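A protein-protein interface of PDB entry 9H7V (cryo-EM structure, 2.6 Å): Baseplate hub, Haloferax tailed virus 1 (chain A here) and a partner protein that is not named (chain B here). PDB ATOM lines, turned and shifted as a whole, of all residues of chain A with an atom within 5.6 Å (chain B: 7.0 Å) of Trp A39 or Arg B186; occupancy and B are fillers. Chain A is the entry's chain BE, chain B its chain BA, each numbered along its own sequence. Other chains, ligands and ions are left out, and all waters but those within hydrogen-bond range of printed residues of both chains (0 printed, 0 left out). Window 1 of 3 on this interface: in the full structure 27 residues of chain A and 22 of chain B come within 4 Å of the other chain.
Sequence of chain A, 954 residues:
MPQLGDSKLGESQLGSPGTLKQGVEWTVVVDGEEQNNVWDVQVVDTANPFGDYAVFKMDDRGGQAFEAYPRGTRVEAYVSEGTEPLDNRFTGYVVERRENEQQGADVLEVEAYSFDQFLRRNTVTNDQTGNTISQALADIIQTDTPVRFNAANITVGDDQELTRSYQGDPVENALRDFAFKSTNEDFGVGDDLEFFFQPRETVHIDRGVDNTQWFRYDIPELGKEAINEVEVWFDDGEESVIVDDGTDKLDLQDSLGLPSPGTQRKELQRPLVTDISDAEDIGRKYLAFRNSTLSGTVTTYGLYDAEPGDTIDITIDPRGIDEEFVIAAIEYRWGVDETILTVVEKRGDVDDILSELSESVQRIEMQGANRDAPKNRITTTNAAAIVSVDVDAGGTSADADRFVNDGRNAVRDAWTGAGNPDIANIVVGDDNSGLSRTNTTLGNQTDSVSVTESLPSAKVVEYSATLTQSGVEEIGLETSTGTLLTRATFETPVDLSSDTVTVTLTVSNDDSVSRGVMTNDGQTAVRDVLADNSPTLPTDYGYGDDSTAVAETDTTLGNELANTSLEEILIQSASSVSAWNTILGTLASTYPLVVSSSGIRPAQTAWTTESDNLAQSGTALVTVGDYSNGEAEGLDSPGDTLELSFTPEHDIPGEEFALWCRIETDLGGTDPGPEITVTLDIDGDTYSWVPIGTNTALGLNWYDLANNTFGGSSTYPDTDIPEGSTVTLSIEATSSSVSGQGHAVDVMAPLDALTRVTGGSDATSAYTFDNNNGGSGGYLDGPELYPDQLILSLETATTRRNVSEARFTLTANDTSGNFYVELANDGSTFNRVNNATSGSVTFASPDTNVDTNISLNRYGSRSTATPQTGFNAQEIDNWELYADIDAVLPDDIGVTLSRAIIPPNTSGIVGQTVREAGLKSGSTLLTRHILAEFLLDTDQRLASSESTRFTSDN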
ATOM      1  N   ASN A  37     -26.997  35.173  -4.236  1.00  0.00           N
ATOM      2  CA  ASN A  37     -25.955  34.184  -4.001  1.00  0.00           C
ATOM      3  C   ASN A  37     -25.825  33.841  -2.514  1.00  0.00           C
ATOM      4  O   ASN A  37     -24.727  33.549  -2.043  1.00  0.00           O
ATOM      5  CB  ASN A  37     -24.637  34.610  -4.663  1.00  0.00           C
ATOM      6  CG  ASN A  37     -24.783  34.972  -6.127  1.00  0.00           C
ATOM      7  OD1 ASN A  37     -25.048  34.110  -6.963  1.00  0.00           O
ATOM      8  ND2 ASN A  37     -24.599  36.242  -6.450  1.00  0.00           N
ATOM      9  N   VAL A  38     -26.956  33.832  -1.792  1.00  0.00           N
ATOM     10  CA  VAL A  38     -26.992  33.565  -0.358  1.00  0.00           C
ATOM     11  C   VAL A  38     -26.921  32.055  -0.131  1.00  0.00           C
ATOM     12  O   VAL A  38     -27.617  31.299  -0.808  1.00  0.00           O
ATOM     13  CB  VAL A  38     -28.248  34.174   0.304  1.00  0.00           C
ATOM     14  CG1 VAL A  38     -28.212  34.061   1.821  1.00  0.00           C
ATOM     15  CG2 VAL A  38     -28.482  35.620  -0.106  1.00  0.00           C
ATOM     16  N   TRP A  39     -26.093  31.632   0.837  1.00  0.00           N
ATOM     17  CA  TRP A  39     -25.919  30.216   1.133  1.00  0.00           C
ATOM     18  C   TRP A  39     -26.116  29.876   2.611  1.00  0.00           C
ATOM     19  O   TRP A  39     -26.242  28.698   2.948  1.00  0.00           O
ATOM     20  CB  TRP A  39     -24.616  29.647   0.549  1.00  0.00           C
ATOM     21  CG  TRP A  39     -23.346  30.366   0.894  1.00  0.00           C
ATOM     22  CD1 TRP A  39     -22.717  31.318   0.147  1.00  0.00           C
ATOM     23  CD2 TRP A  39     -22.505  30.143   2.042  1.00  0.00           C
ATOM     24  NE1 TRP A  39     -21.562  31.721   0.757  1.00  0.00           N
ATOM     25  CE2 TRP A  39     -21.403  31.020   1.922  1.00  0.00           C
ATOM     26  CE3 TRP A  39     -22.577  29.306   3.164  1.00  0.00           C
ATOM     27  CZ2 TRP A  39     -20.390  31.080   2.880  1.00  0.00           C
ATOM     28  CZ3 TRP A  39     -21.575  29.365   4.109  1.00  0.00           C
ATOM     29  CH2 TRP A  39     -20.496  30.241   3.967  1.00  0.00           C
ATOM     30  N   ASP A  40     -26.152  30.896   3.483  1.00  0.00           N
ATOM     31  CA  ASP A  40     -26.496  30.700   4.886  1.00  0.00           C
ATOM     32  C   ASP A  40     -27.071  31.980   5.490  1.00  0.00           C
ATOM     33  O   ASP A  40     -26.684  33.083   5.107  1.00  0.00           O
ATOM     34  CB  ASP A  40     -25.322  30.165   5.715  1.00  0.00           C
ATOM     35  CG  ASP A  40     -25.745  29.356   6.933  1.00  0.00           C
ATOM     36  OD1 ASP A  40     -26.966  29.213   7.161  1.00  0.00           O
ATOM     37  OD2 ASP A  40     -24.847  28.868   7.647  1.00  0.00           O
ATOM     38  N   VAL A  41     -27.993  31.795   6.447  1.00  0.00           N
ATOM     39  CA  VAL A  41     -28.658  32.862   7.182  1.00  0.00           C
ATOM     40  C   VAL A  41     -28.751  32.455   8.653  1.00  0.00           C
ATOM     41  O   VAL A  41     -29.147  31.332   8.967  1.00  0.00           O
ATOM     42  CB  VAL A  41     -30.055  33.175   6.597  1.00  0.00           C
ATOM     43  CG1 VAL A  41     -30.867  34.116   7.476  1.00  0.00           C
ATOM     44  CG2 VAL A  41     -29.994  33.719   5.178  1.00  0.00           C
ATOM     45  N   LYS A  57     -24.516  35.035   4.798  1.00  0.00           N
ATOM     46  CA  LYS A  57     -23.311  34.612   4.102  1.00  0.00           C
ATOM     47  C   LYS A  57     -23.631  34.416   2.623  1.00  0.00           C
ATOM     48  O   LYS A  57     -24.583  33.718   2.275  1.00  0.00           O
ATOM     49  CB  LYS A  57     -22.710  33.359   4.748  1.00  0.00           C
ATOM     50  CG  LYS A  57     -22.059  33.571   6.109  1.00  0.00           C
ATOM     51  CD  LYS A  57     -21.718  32.275   6.807  1.00  0.00           C
ATOM     52  CE  LYS A  57     -21.295  32.459   8.248  1.00  0.00           C
ATOM     53  NZ  LYS A  57     -19.860  32.817   8.357  1.00  0.00           N
ATOM     54  N   MET A  58     -22.820  35.054   1.770  1.00  0.00           N
ATOM     55  CA  MET A  58     -23.027  35.095   0.330  1.00  0.00           C
ATOM     56  C   MET A  58     -21.714  34.816  -0.396  1.00  0.00           C
ATOM     57  O   MET A  58     -20.636  34.921   0.189  1.00  0.00           O
ATOM     58  CB  MET A  58     -23.534  36.474  -0.109  1.00  0.00           C
ATOM     59  CG  MET A  58     -24.955  36.771   0.319  1.00  0.00           C
ATOM     60  SD  MET A  58     -25.159  38.464   0.925  1.00  0.00           S
ATOM     61  CE  MET A  58     -24.258  38.378   2.470  1.00  0.00           C
ATOM     62  N   ASP A  59     -21.834  34.458  -1.681  1.00  0.00           N
ATOM     63  CA  ASP A  59     -20.713  34.401  -2.604  1.00  0.00           C
ATOM     64  C   ASP A  59     -20.659  35.693  -3.410  1.00  0.00           C
ATOM     65  O   ASP A  59     -21.685  36.186  -3.878  1.00  0.00           O
ATOM     66  CB  ASP A  59     -20.811  33.197  -3.542  1.00  0.00           C
ATOM     67  CG  ASP A  59     -20.210  31.923  -2.975  1.00  0.00           C
ATOM     68  OD1 ASP A  59     -18.990  31.913  -2.713  1.00  0.00           O
ATOM     69  OD2 ASP A  59     -20.966  30.953  -2.801  1.00  0.00           O
ATOM     70  N   GLN A 102     -11.732  32.381   1.637  1.00  0.00           N
ATOM     71  CA  GLN A 102     -11.957  31.136   2.356  1.00  0.00           C
ATOM     72  C   GLN A 102     -11.718  29.965   1.408  1.00  0.00           C
ATOM     73  O   GLN A 102     -12.648  29.502   0.748  1.00  0.00           O
ATOM     74  CB  GLN A 102     -13.361  31.086   2.963  1.00  0.00           C
ATOM     75  CG  GLN A 102     -13.578  32.068   4.108  1.00  0.00           C
ATOM     76  CD  GLN A 102     -14.780  31.768   4.971  1.00  0.00           C
ATOM     77  OE1 GLN A 102     -15.259  30.637   5.047  1.00  0.00           O
ATOM     78  NE2 GLN A 102     -15.273  32.791   5.651  1.00  0.00           N
ATOM     79  N   VAL A 107     -16.031  35.174   0.213  1.00  0.00           N
ATOM     80  CA  VAL A 107     -17.212  35.042   1.052  1.00  0.00           C
ATOM     81  C   VAL A 107     -17.585  36.411   1.613  1.00  0.00           C
ATOM     82  O   VAL A 107     -16.811  37.011   2.355  1.00  0.00           O
ATOM     83  CB  VAL A 107     -16.998  33.998   2.168  1.00  0.00           C
ATOM     84  CG1 VAL A 107     -18.147  33.968   3.167  1.00  0.00           C
ATOM     85  CG2 VAL A 107     -16.745  32.605   1.611  1.00  0.00           C
ATOM     86  N   TRP A 334     -30.398  28.643   9.011  1.00  0.00           N
ATOM     87  CA  TRP A 334     -30.498  27.899   7.766  1.00  0.00           C
ATOM     88  C   TRP A 334     -29.285  26.976   7.670  1.00  0.00           C
ATOM     89  O   TRP A 334     -28.398  27.027   8.521  1.00  0.00           O
ATOM     90  CB  TRP A 334     -30.554  28.908   6.614  1.00  0.00           C
ATOM     91  CG  TRP A 334     -31.285  28.509   5.366  1.00  0.00           C
ATOM     92  CD1 TRP A 334     -32.199  27.510   5.189  1.00  0.00           C
ATOM     93  CD2 TRP A 334     -31.191  29.187   4.101  1.00  0.00           C
ATOM     94  NE1 TRP A 334     -32.653  27.502   3.896  1.00  0.00           N
ATOM     95  CE2 TRP A 334     -32.056  28.522   3.204  1.00  0.00           C
ATOM     96  CE3 TRP A 334     -30.449  30.282   3.641  1.00  0.00           C
ATOM     97  CZ2 TRP A 334     -32.193  28.920   1.873  1.00  0.00           C
ATOM     98  CZ3 TRP A 334     -30.584  30.675   2.326  1.00  0.00           C
ATOM     99  CH2 TRP A 334     -31.445  30.001   1.457  1.00  0.00           C
ATOM    100  N   GLY A 335     -29.248  26.118   6.645  1.00  0.00           N
ATOM    101  CA  GLY A 335     -28.097  25.256   6.424  1.00  0.00           C
ATOM    102  C   GLY A 335     -28.108  24.029   7.333  1.00  0.00           C
ATOM    103  O   GLY A 335     -28.133  22.901   6.843  1.00  0.00           O
ATOM    104  N   VAL A 336     -28.075  24.268   8.652  1.00  0.00           N
ATOM    105  CA  VAL A 336     -28.169  23.222   9.662  1.00  0.00           C
ATOM    106  C   VAL A 336     -29.638  22.957   9.992  1.00  0.00           C
ATOM    107  O   VAL A 336     -29.956  21.954  10.631  1.00  0.00           O
ATOM    108  CB  VAL A 336     -27.343  23.545  10.926  1.00  0.00           C
ATOM    109  CG1 VAL A 336     -25.847  23.407  10.687  1.00  0.00           C
ATOM    110  CG2 VAL A 336     -27.673  24.904  11.527  1.00  0.00           C
ATOM    111  N   GLU B  34     -26.346  17.770   1.623  1.00  0.00           N
ATOM    112  CA  GLU B  34     -26.908  18.865   2.398  1.00  0.00           C
ATOM    113  C   GLU B  34     -28.161  18.452   3.172  1.00  0.00           C
ATOM    114  O   GLU B  34     -28.809  19.315   3.763  1.00  0.00           O
ATOM    115  CB  GLU B  34     -27.195  20.073   1.501  1.00  0.00           C
ATOM    116  CG  GLU B  34     -25.973  20.656   0.806  1.00  0.00           C
ATOM    117  CD  GLU B  34     -24.832  21.138   1.690  1.00  0.00           C
ATOM    118  OE1 GLU B  34     -25.104  21.686   2.780  1.00  0.00           O
ATOM    119  OE2 GLU B  34     -23.667  20.961   1.285  1.00  0.00           O
ATOM    120  N   ASN B  36     -30.017  17.390   6.309  1.00  0.00           N
ATOM    121  CA  ASN B  36     -29.829  17.385   7.747  1.00  0.00           C
ATOM    122  C   ASN B  36     -30.635  16.233   8.335  1.00  0.00           C
ATOM    123  O   ASN B  36     -31.863  16.238   8.291  1.00  0.00           O
ATOM    124  CB  ASN B  36     -30.161  18.738   8.381  1.00  0.00           C
ATOM    125  CG  ASN B  36     -29.289  19.865   7.873  1.00  0.00           C
ATOM    126  OD1 ASN B  36     -28.094  19.915   8.160  1.00  0.00           O
ATOM    127  ND2 ASN B  36     -29.879  20.780   7.124  1.00  0.00           N
ATOM    128  N   TRP B  52     -31.991  21.593  -0.318  1.00  0.00           N
ATOM    129  CA  TRP B  52     -30.918  22.133  -1.137  1.00  0.00           C
ATOM    130  C   TRP B  52     -30.679  21.262  -2.370  1.00  0.00           C
ATOM    131  O   TRP B  52     -31.215  20.160  -2.473  1.00  0.00           O
ATOM    132  CB  TRP B  52     -29.632  22.231  -0.308  1.00  0.00           C
ATOM    133  CG  TRP B  52     -29.705  23.074   0.928  1.00  0.00           C
ATOM    134  CD1 TRP B  52     -29.963  22.652   2.200  1.00  0.00           C
ATOM    135  CD2 TRP B  52     -29.464  24.488   1.017  1.00  0.00           C
ATOM    136  NE1 TRP B  52     -29.918  23.706   3.071  1.00  0.00           N
ATOM    137  CE2 TRP B  52     -29.613  24.846   2.376  1.00  0.00           C
ATOM    138  CE3 TRP B  52     -29.150  25.486   0.086  1.00  0.00           C
ATOM    139  CZ2 TRP B  52     -29.456  26.161   2.818  1.00  0.00           C
ATOM    140  CZ3 TRP B  52     -28.990  26.783   0.524  1.00  0.00           C
ATOM    141  CH2 TRP B  52     -29.141  27.112   1.873  1.00  0.00           C
ATOM    142  N   SER B  53     -29.841  21.781  -3.281  1.00  0.00           N
ATOM    143  CA  SER B  53     -29.322  21.074  -4.442  1.00  0.00           C
ATOM    144  C   SER B  53     -28.633  19.776  -4.028  1.00  0.00           C
ATOM    145  O   SER B  53     -27.994  19.713  -2.979  1.00  0.00           O
ATOM    146  CB  SER B  53     -28.380  21.956  -5.221  1.00  0.00           C
ATOM    147  OG  SER B  53     -27.369  22.488  -4.378  1.00  0.00           O
ATOM    148  N   GLY B  54     -28.778  18.751  -4.875  1.00  0.00           N
ATOM    149  CA  GLY B  54     -28.068  17.493  -4.708  1.00  0.00           C
ATOM    150  C   GLY B  54     -26.655  17.571  -5.278  1.00  0.00           C
ATOM    151  O   GLY B  54     -26.159  18.655  -5.581  1.00  0.00           O
ATOM    152  N   VAL B 184     -17.945  25.217  -5.612  1.00  0.00           N
ATOM    153  CA  VAL B 184     -19.239  24.661  -5.970  1.00  0.00           C
ATOM    154  C   VAL B 184     -20.113  24.744  -4.719  1.00  0.00           C
ATOM    155  O   VAL B 184     -19.753  24.194  -3.679  1.00  0.00           O
ATOM    156  CB  VAL B 184     -19.101  23.226  -6.524  1.00  0.00           C
ATOM    157  CG1 VAL B 184     -20.444  22.546  -6.716  1.00  0.00           C
ATOM    158  CG2 VAL B 184     -18.309  23.194  -7.822  1.00  0.00           C
ATOM    159  N   ARG B 185     -21.248  25.449  -4.830  1.00  0.00           N
ATOM    160  CA  ARG B 185     -22.009  25.866  -3.660  1.00  0.00           C
ATOM    161  C   ARG B 185     -23.481  25.492  -3.777  1.00  0.00           C
ATOM    162  O   ARG B 185     -24.066  25.563  -4.855  1.00  0.00           O
ATOM    163  CB  ARG B 185     -21.848  27.369  -3.422  1.00  0.00           C
ATOM    164  CG  ARG B 185     -20.711  27.711  -2.471  1.00  0.00           C
ATOM    165  CD  ARG B 185     -21.163  27.970  -1.046  1.00  0.00           C
ATOM    166  NE  ARG B 185     -20.047  27.948  -0.107  1.00  0.00           N
ATOM    167  CZ  ARG B 185     -19.096  28.875  -0.005  1.00  0.00           C
ATOM    168  NH1 ARG B 185     -18.137  28.731   0.893  1.00  0.00           N
ATOM    169  NH2 ARG B 185     -19.091  29.934  -0.796  1.00  0.00           N
ATOM    170  N   ARG B 186     -24.059  25.137  -2.621  1.00  0.00           N
ATOM    171  CA  ARG B 186     -25.460  24.774  -2.481  1.00  0.00           C
ATOM    172  C   ARG B 186     -26.343  25.978  -2.800  1.00  0.00           C
ATOM    173  O   ARG B 186     -26.020  27.114  -2.451  1.00  0.00           O
ATOM    174  CB  ARG B 186     -25.743  24.206  -1.085  1.00  0.00           C
ATOM    175  CG  ARG B 186     -25.607  25.204   0.058  1.00  0.00           C
ATOM    176  CD  ARG B 186     -25.892  24.598   1.417  1.00  0.00           C
ATOM    177  NE  ARG B 186     -25.765  25.604   2.462  1.00  0.00           N
ATOM    178  CZ  ARG B 186     -25.321  25.389   3.696  1.00  0.00           C
ATOM    179  NH1 ARG B 186     -25.253  26.395   4.552  1.00  0.00           N
ATOM    180  NH2 ARG B 186     -24.931  24.183   4.074  1.00  0.00           N
ATOM    181  N   VAL B 187     -27.446  25.697  -3.495  1.00  0.00           N
ATOM    182  CA  VAL B 187     -28.505  26.659  -3.736  1.00  0.00           C
ATOM    183  C   VAL B 187     -29.821  26.012  -3.311  1.00  0.00           C
ATOM    184  O   VAL B 187     -29.967  24.797  -3.434  1.00  0.00           O
ATOM    185  CB  VAL B 187     -28.532  27.136  -5.203  1.00  0.00           C
ATOM    186  CG1 VAL B 187     -27.567  28.287  -5.441  1.00  0.00           C
ATOM    187  CG2 VAL B 187     -28.262  26.010  -6.187  1.00  0.00           C
ATOM    188  N   PRO B 188     -30.806  26.774  -2.778  1.00  0.00           N
ATOM    189  CA  PRO B 188     -32.108  26.198  -2.440  1.00  0.00           C
ATOM    190  C   PRO B 188     -32.915  25.946  -3.712  1.00  0.00           C
ATOM    191  O   PRO B 188     -32.639  26.559  -4.743  1.00  0.00           O
ATOM    192  CB  PRO B 188     -32.765  27.303  -1.597  1.00  0.00           C
ATOM    193  CG  PRO B 188     -32.154  28.586  -2.117  1.00  0.00           C
ATOM    194  CD  PRO B 188     -30.730  28.215  -2.476  1.00  0.00           C
ATOM    195  N   ASP B 192     -29.260  21.380  -8.964  1.00  0.00           N
ATOM    196  CA  ASP B 192     -27.824  21.425  -9.205  1.00  0.00           C
ATOM    197  C   ASP B 192     -27.183  22.653  -8.561  1.00  0.00           C
ATOM    198  O   ASP B 192     -27.789  23.723  -8.532  1.00  0.00           O
ATOM    199  CB  ASP B 192     -27.517  21.373 -10.703  1.00  0.00           C
ATOM    200  CG  ASP B 192     -27.828  20.034 -11.347  1.00  0.00           C
ATOM    201  OD1 ASP B 192     -27.362  19.000 -10.823  1.00  0.00           O
ATOM    202  OD2 ASP B 192     -28.532  20.036 -12.374  1.00  0.00           O
ATOM    203  N   PRO B 193     -25.929  22.535  -8.058  1.00  0.00           N
ATOM    204  CA  PRO B 193     -25.236  23.648  -7.405  1.00  0.00           C
ATOM    205  C   PRO B 193     -24.727  24.740  -8.345  1.00  0.00           C
ATOM    206  O   PRO B 193     -24.743  24.583  -9.565  1.00  0.00           O
ATOM    207  CB  PRO B 193     -24.048  22.941  -6.737  1.00  0.00           C
ATOM    208  CG  PRO B 193     -23.744  21.800  -7.671  1.00  0.00           C
ATOM    209  CD  PRO B 193     -25.116  21.307  -8.070  1.00  0.00           C
ATOM    210  N   ARG B 194     -24.271  25.838  -7.731  1.00  0.00           N
ATOM    211  CA  ARG B 194     -23.734  27.014  -8.394  1.00  0.00           C
ATOM    212  C   ARG B 194     -22.215  26.880  -8.482  1.00  0.00           C
ATOM    213  O   ARG B 194     -21.572  26.452  -7.526  1.00  0.00           O
ATOM    214  CB  ARG B 194     -24.176  28.249  -7.602  1.00  0.00           C
ATOM    215  CG  ARG B 194     -23.514  29.565  -7.986  1.00  0.00           C
ATOM    216  CD  ARG B 194     -24.209  30.763  -7.359  1.00  0.00           C
ATOM    217  NE  ARG B 194     -24.681  30.551  -5.992  1.00  0.00           N
ATOM    218  CZ  ARG B 194     -23.929  30.601  -4.896  1.00  0.00           C
ATOM    219  NH1 ARG B 194     -24.476  30.387  -3.713  1.00  0.00           N
ATOM    220  NH2 ARG B 194     -22.635  30.854  -4.982  1.00  0.00           N
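The backbone carbonyl oxygen (O) of Gly A335 lies within hydrogen-bond range of the side-chain amide nitrogen (ND2) of Asn B36 (2.8 Å).
The side-chain carboxylate (OD1) of Asp A59 lies within salt-bridge range of the guanidinium group (NH2) of Arg B185, at 2.8 Å.
The backbone carbonyl oxygen (O) of Trp A39 sits at hydrogen-bond distance from the guanidinium group (NH1) of Arg B186 (3.0 Å).
NH1 of Arg B186 is in salt-bridge range of OD2 of Asp A40 (3.98 Å).
NH2 of Arg B194 lies within salt-bridge range of OD2 of Asp A59 (2.7 Å).
The guanidinium group (NH2) of Arg B185 lies close to the indole nitrogen (NE1) of Trp A39, 3.4 Å away.
Of the 13 printed residues of chain B, 6 touch a printed residue of chain A.
Hydrophobic or aromatic side chains of chain A that line the printed part of chain B: Trp A39 and Trp A334.
Among the printed residues, 13 pairs touch across the chains.
Among the printed residues, Asp or Glu carboxylates within 4 Å of a Lys or Arg side-chain nitrogen of the other chain: Asp A40 with Arg B186 (3.98 Å), Asp A59 with Arg B185 (2.8 Å) and Asp A59 with Arg B194 (2.7 Å).
Trp A39 touches three residues of chain B.
Of chain A, only Trp A39 (3.0 Å), Asp A40 (3.8 Å) and Gly A335 (3.6 Å) come within 4 Å of Arg B186.
Of the printed residues of chain B, Asp A59 touches Arg B185 and Arg B194.
Printed residues of chain A within 4 Å of Trp B52: Trp A39 (3.5 Å), Trp A334 (3.5 Å) and Gly A335 (3.8 Å).
Printed residues of chain B within 4 Å of Gly A335: Asn B36 (2.8 Å), Trp B52 (3.8 Å) and Arg B186 (3.6 Å).
Gly B54 touches none of the printed residues of chain A.
The nearest residue of chain A that does not touch Arg B186 is Val A38 (4.8 Å).
The nearest printed residue of chain A that does not touch Trp B52 is Val A38 (4.9 Å).
The side-chain carboxylate (OE1) of Glu B34 is in salt-bridge range of the guanidinium group (NH2) of Arg B186, at 2.8 Å.
N of Arg B185 lies within hydrogen-bond range of O of Arg B194 (2.9 Å).
O of Asn A37 lies within hydrogen-bond range of N of Asp A59 (3.1 Å).
NE1 of Trp A39 sits close to O of Met A58 (3.4 Å).
The backbone carbonyl oxygen of Asp A40 lies within hydrogen-bond range of the backbone NH of Lys A57, at 2.9 Å.
N of Trp A334 is in hydrogen-bond range of O of Val A41 (3.0 Å).
Among the printed residues, pairs that only touch across the chains: Asn A37 with Arg B194 (3.5 Å), Trp A39 with Trp B52 (3.5 Å), Trp A334 with Trp B52 (3.5 Å), Val A336 with Asn B36 (3.5 Å), Gly A335 with Arg B186 (3.6 Å), Gly A335 with Trp B52 (3.8 Å) and Trp A334 with Pro B188 (3.9 Å).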
